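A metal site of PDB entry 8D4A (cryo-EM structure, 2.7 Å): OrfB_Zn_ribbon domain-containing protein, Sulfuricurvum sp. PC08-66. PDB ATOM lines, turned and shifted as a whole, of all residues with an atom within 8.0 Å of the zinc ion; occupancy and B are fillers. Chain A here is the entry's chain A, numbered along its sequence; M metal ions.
N of Lys 1175 sits close to SG of Cys 1173, 3.7 Å away. SG of Cys 1170 sits close to N of Val 1172. The backbone NH (N) of Cys 1170 lies within hydrogen-bond range of the backbone carbonyl oxygen (O) of Lys 1175, at 2.8 Å. N of Phe 1193 lies close to SG of Cys 1191. The backbone carbonyl oxygen (O) of Phe 1193 is in hydrogen-bond range of the backbone NH (N) of Cys 1188, at 2.8 Å. The side-chain sulfur (SG) of Cys 1188 sits close to the backbone NH (N) of Glu 1190 (3.5 Å).
Along chain A the residues within 4 Å of the zinc ion span positions 1170 to 1191. The nearest printed residue that does not touch the zinc ion is Phe 1193 (4.3 Å).
The zinc ion is bound by the side-chain sulfur (SG) of Cys 1173 (2.3 Å), the side-chain sulfur (SG) of Cys 1170 (2.3 Å), the side-chain sulfur (SG) of Cys 1191 (2.3 Å) and the side-chain sulfur (SG) of Cys 1188 (2.3 Å). The zinc ion has four donor atoms within binding distance.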
ATOM      1  N   LYS A1169     -15.215   6.090  25.909  1.00  0.00           N
ATOM      2  CA  LYS A1169     -16.617   6.434  26.127  1.00  0.00           C
ATOM      3  C   LYS A1169     -16.681   7.840  26.688  1.00  0.00           C
ATOM      4  O   LYS A1169     -15.791   8.266  27.433  1.00  0.00           O
ATOM      5  CB  LYS A1169     -17.314   5.440  27.066  1.00  0.00           C
ATOM      6  CG  LYS A1169     -18.825   5.590  27.099  1.00  0.00           C
ATOM      7  CD  LYS A1169     -19.509   4.491  27.871  1.00  0.00           C
ATOM      8  CE  LYS A1169     -19.558   3.224  27.064  1.00  0.00           C
ATOM      9  NZ  LYS A1169     -20.270   2.144  27.812  1.00  0.00           N
ATOM     10  N   CYS A1170     -17.721   8.568  26.303  1.00  0.00           N
ATOM     11  CA  CYS A1170     -17.874   9.927  26.801  1.00  0.00           C
ATOM     12  C   CYS A1170     -18.581   9.907  28.155  1.00  0.00           C
ATOM     13  O   CYS A1170     -19.576   9.206  28.311  1.00  0.00           O
ATOM     14  CB  CYS A1170     -18.662  10.788  25.819  1.00  0.00           C
ATOM     15  SG  CYS A1170     -18.753  12.518  26.300  1.00  0.00           S
ATOM     16  N   PRO A1171     -18.082  10.653  29.150  1.00  0.00           N
ATOM     17  CA  PRO A1171     -18.779  10.718  30.434  1.00  0.00           C
ATOM     18  C   PRO A1171     -20.150  11.368  30.347  1.00  0.00           C
ATOM     19  O   PRO A1171     -20.994  11.134  31.226  1.00  0.00           O
ATOM     20  CB  PRO A1171     -17.829  11.545  31.308  1.00  0.00           C
ATOM     21  CG  PRO A1171     -16.517  11.443  30.635  1.00  0.00           C
ATOM     22  CD  PRO A1171     -16.799  11.353  29.187  1.00  0.00           C
ATOM     23  N   VAL A1172     -20.397  12.192  29.328  1.00  0.00           N
ATOM     24  CA  VAL A1172     -21.639  12.956  29.226  1.00  0.00           C
ATOM     25  C   VAL A1172     -22.675  12.207  28.395  1.00  0.00           C
ATOM     26  O   VAL A1172     -23.739  11.841  28.896  1.00  0.00           O
ATOM     27  CB  VAL A1172     -21.358  14.344  28.638  1.00  0.00           C
ATOM     28  CG1 VAL A1172     -22.644  15.136  28.505  1.00  0.00           C
ATOM     29  CG2 VAL A1172     -20.362  15.089  29.497  1.00  0.00           C
ATOM     30  N   CYS A1173     -22.369  11.984  27.112  1.00  0.00           N
ATOM     31  CA  CYS A1173     -23.330  11.424  26.181  1.00  0.00           C
ATOM     32  C   CYS A1173     -23.222   9.914  26.007  1.00  0.00           C
ATOM     33  O   CYS A1173     -24.040   9.327  25.300  1.00  0.00           O
ATOM     34  CB  CYS A1173     -23.206  12.111  24.818  1.00  0.00           C
ATOM     35  SG  CYS A1173     -21.624  11.883  23.997  1.00  0.00           S
ATOM     36  N   SER A1174     -22.227   9.286  26.645  1.00  0.00           N
ATOM     37  CA  SER A1174     -21.962   7.848  26.581  1.00  0.00           C
ATOM     38  C   SER A1174     -21.698   7.340  25.173  1.00  0.00           C
ATOM     39  O   SER A1174     -21.880   6.145  24.900  1.00  0.00           O
ATOM     40  CB  SER A1174     -23.095   7.031  27.225  1.00  0.00           C
ATOM     41  OG  SER A1174     -23.308   7.449  28.566  1.00  0.00           O
ATOM     42  N   LYS A1175     -21.269   8.207  24.260  1.00  0.00           N
ATOM     43  CA  LYS A1175     -20.885   7.771  22.935  1.00  0.00           C
ATOM     44  C   LYS A1175     -19.399   7.438  22.902  1.00  0.00           C
ATOM     45  O   LYS A1175     -18.608   7.987  23.668  1.00  0.00           O
ATOM     46  CB  LYS A1175     -21.213   8.839  21.899  1.00  0.00           C
ATOM     47  CG  LYS A1175     -22.681   9.187  21.808  1.00  0.00           C
ATOM     48  CD  LYS A1175     -23.487   8.047  21.234  1.00  0.00           C
ATOM     49  CE  LYS A1175     -24.961   8.419  21.159  1.00  0.00           C
ATOM     50  NZ  LYS A1175     -25.213   9.497  20.163  1.00  0.00           N
ATOM     51  N   THR A1176     -19.032   6.547  22.003  1.00  0.00           N
ATOM     52  CA  THR A1176     -17.669   6.046  21.928  1.00  0.00           C
ATOM     53  C   THR A1176     -16.839   6.693  20.844  1.00  0.00           C
ATOM     54  O   THR A1176     -15.738   6.217  20.552  1.00  0.00           O
ATOM     55  CB  THR A1176     -17.674   4.522  21.733  1.00  0.00           C
ATOM     56  OG1 THR A1176     -18.171   4.216  20.428  1.00  0.00           O
ATOM     57  CG2 THR A1176     -18.554   3.876  22.763  1.00  0.00           C
ATOM     58  N   ASN A1177     -17.333   7.773  20.227  1.00  0.00           N
ATOM     59  CA  ASN A1177     -16.565   8.484  19.198  1.00  0.00           C
ATOM     60  C   ASN A1177     -15.749   9.570  19.891  1.00  0.00           C
ATOM     61  O   ASN A1177     -15.997  10.769  19.740  1.00  0.00           O
ATOM     62  CB  ASN A1177     -17.497   9.055  18.137  1.00  0.00           C
ATOM     63  CG  ASN A1177     -16.760   9.619  16.928  1.00  0.00           C
ATOM     64  OD1 ASN A1177     -15.536   9.610  16.881  1.00  0.00           O
ATOM     65  ND2 ASN A1177     -17.509  10.099  15.951  1.00  0.00           N
ATOM     66  N   VAL A1178     -14.768   9.131  20.674  1.00  0.00           N
ATOM     67  CA  VAL A1178     -13.910  10.012  21.440  1.00  0.00           C
ATOM     68  C   VAL A1178     -12.464   9.703  21.095  1.00  0.00           C
ATOM     69  O   VAL A1178     -12.161   8.690  20.466  1.00  0.00           O
ATOM     70  CB  VAL A1178     -14.118   9.885  22.966  1.00  0.00           C
ATOM     71  CG1 VAL A1178     -15.585  10.053  23.330  1.00  0.00           C
ATOM     72  CG2 VAL A1178     -13.605   8.554  23.456  1.00  0.00           C
ATOM     73  N   LEU A1186      -9.189  13.858  27.289  1.00  0.00           N
ATOM     74  CA  LEU A1186     -10.298  13.203  26.601  1.00  0.00           C
ATOM     75  C   LEU A1186     -11.157  14.236  25.886  1.00  0.00           C
ATOM     76  O   LEU A1186     -11.630  15.199  26.485  1.00  0.00           O
ATOM     77  CB  LEU A1186     -11.148  12.416  27.596  1.00  0.00           C
ATOM     78  CG  LEU A1186     -12.288  11.634  26.965  1.00  0.00           C
ATOM     79  CD1 LEU A1186     -11.747  10.429  26.226  1.00  0.00           C
ATOM     80  CD2 LEU A1186     -13.273  11.228  28.023  1.00  0.00           C
ATOM     81  N   VAL A1187     -11.342  14.028  24.588  1.00  0.00           N
ATOM     82  CA  VAL A1187     -12.135  14.923  23.741  1.00  0.00           C
ATOM     83  C   VAL A1187     -13.220  14.092  23.062  1.00  0.00           C
ATOM     84  O   VAL A1187     -12.931  13.047  22.475  1.00  0.00           O
ATOM     85  CB  VAL A1187     -11.266  15.636  22.687  1.00  0.00           C
ATOM     86  CG1 VAL A1187     -12.105  16.601  21.869  1.00  0.00           C
ATOM     87  CG2 VAL A1187     -10.118  16.365  23.339  1.00  0.00           C
ATOM     88  N   CYS A1188     -14.459  14.555  23.148  1.00  0.00           N
ATOM     89  CA  CYS A1188     -15.585  13.895  22.487  1.00  0.00           C
ATOM     90  C   CYS A1188     -15.896  14.603  21.184  1.00  0.00           C
ATOM     91  O   CYS A1188     -16.031  15.829  21.151  1.00  0.00           O
ATOM     92  CB  CYS A1188     -16.831  13.878  23.373  1.00  0.00           C
ATOM     93  SG  CYS A1188     -18.230  13.037  22.622  1.00  0.00           S
ATOM     94  N   LYS A1189     -16.000  13.815  20.104  1.00  0.00           N
ATOM     95  CA  LYS A1189     -16.238  14.390  18.792  1.00  0.00           C
ATOM     96  C   LYS A1189     -17.710  14.581  18.479  1.00  0.00           C
ATOM     97  O   LYS A1189     -18.049  15.127  17.422  1.00  0.00           O
ATOM     98  CB  LYS A1189     -15.596  13.501  17.722  1.00  0.00           C
ATOM     99  CG  LYS A1189     -14.096  13.297  17.907  1.00  0.00           C
ATOM    100  CD  LYS A1189     -13.501  12.453  16.780  1.00  0.00           C
ATOM    101  CE  LYS A1189     -13.985  12.909  15.404  1.00  0.00           C
ATOM    102  NZ  LYS A1189     -13.004  12.602  14.328  1.00  0.00           N
ATOM    103  N   GLU A1190     -18.612  14.159  19.367  1.00  0.00           N
ATOM    104  CA  GLU A1190     -20.041  14.229  19.096  1.00  0.00           C
ATOM    105  C   GLU A1190     -20.822  15.104  20.068  1.00  0.00           C
ATOM    106  O   GLU A1190     -22.015  15.310  19.855  1.00  0.00           O
ATOM    107  CB  GLU A1190     -20.645  12.830  19.067  1.00  0.00           C
ATOM    108  CG  GLU A1190     -20.157  11.992  17.907  1.00  0.00           C
ATOM    109  CD  GLU A1190     -20.743  10.603  17.906  1.00  0.00           C
ATOM    110  OE1 GLU A1190     -21.446  10.255  18.876  1.00  0.00           O
ATOM    111  OE2 GLU A1190     -20.507   9.865  16.925  1.00  0.00           O
ATOM    112  N   CYS A1191     -20.208  15.593  21.128  1.00  0.00           N
ATOM    113  CA  CYS A1191     -20.894  16.555  21.987  1.00  0.00           C
ATOM    114  C   CYS A1191     -19.995  17.676  22.472  1.00  0.00           C
ATOM    115  O   CYS A1191     -20.468  18.529  23.223  1.00  0.00           O
ATOM    116  CB  CYS A1191     -21.538  15.847  23.186  1.00  0.00           C
ATOM    117  SG  CYS A1191     -20.414  15.478  24.561  1.00  0.00           S
ATOM    118  N   GLY A1192     -18.726  17.729  22.067  1.00  0.00           N
ATOM    119  CA  GLY A1192     -17.838  18.798  22.455  1.00  0.00           C
ATOM    120  C   GLY A1192     -17.263  18.705  23.848  1.00  0.00           C
ATOM    121  O   GLY A1192     -16.700  19.693  24.331  1.00  0.00           O
ATOM    122  N   PHE A1193     -17.393  17.557  24.513  1.00  0.00           N
ATOM    123  CA  PHE A1193     -16.825  17.405  25.845  1.00  0.00           C
ATOM    124  C   PHE A1193     -15.306  17.392  25.788  1.00  0.00           C
ATOM    125  O   PHE A1193     -14.698  16.752  24.925  1.00  0.00           O
ATOM    126  CB  PHE A1193     -17.342  16.110  26.490  1.00  0.00           C
ATOM    127  CG  PHE A1193     -16.650  15.755  27.776  1.00  0.00           C
ATOM    128  CD1 PHE A1193     -16.997  16.370  28.964  1.00  0.00           C
ATOM    129  CD2 PHE A1193     -15.655  14.781  27.802  1.00  0.00           C
ATOM    130  CE1 PHE A1193     -16.373  16.030  30.145  1.00  0.00           C
ATOM    131  CE2 PHE A1193     -15.034  14.455  28.980  1.00  0.00           C
ATOM    132  CZ  PHE A1193     -15.390  15.078  30.142  1.00  0.00           C
ATOM    133  N   ARG A1194     -14.682  18.135  26.703  1.00  0.00           N
ATOM    134  CA  ARG A1194     -13.237  18.150  26.863  1.00  0.00           C
ATOM    135  C   ARG A1194     -12.898  18.088  28.341  1.00  0.00           C
ATOM    136  O   ARG A1194     -13.530  18.771  29.146  1.00  0.00           O
ATOM    137  CB  ARG A1194     -12.617  19.396  26.232  1.00  0.00           C
ATOM    138  CG  ARG A1194     -12.645  19.413  24.711  1.00  0.00           C
ATOM    139  CD  ARG A1194     -11.865  20.594  24.164  1.00  0.00           C
ATOM    140  NE  ARG A1194     -10.434  20.468  24.410  1.00  0.00           N
ATOM    141  CZ  ARG A1194      -9.560  20.053  23.498  1.00  0.00           C
ATOM    142  NH1 ARG A1194      -9.965  19.741  22.286  1.00  0.00           N
ATOM    143  NH2 ARG A1194      -8.272  19.955  23.814  1.00  0.00           N
HETATM  144 ZN    ZN M   1     -19.783  13.248  24.346  1.00  0.00          ZN
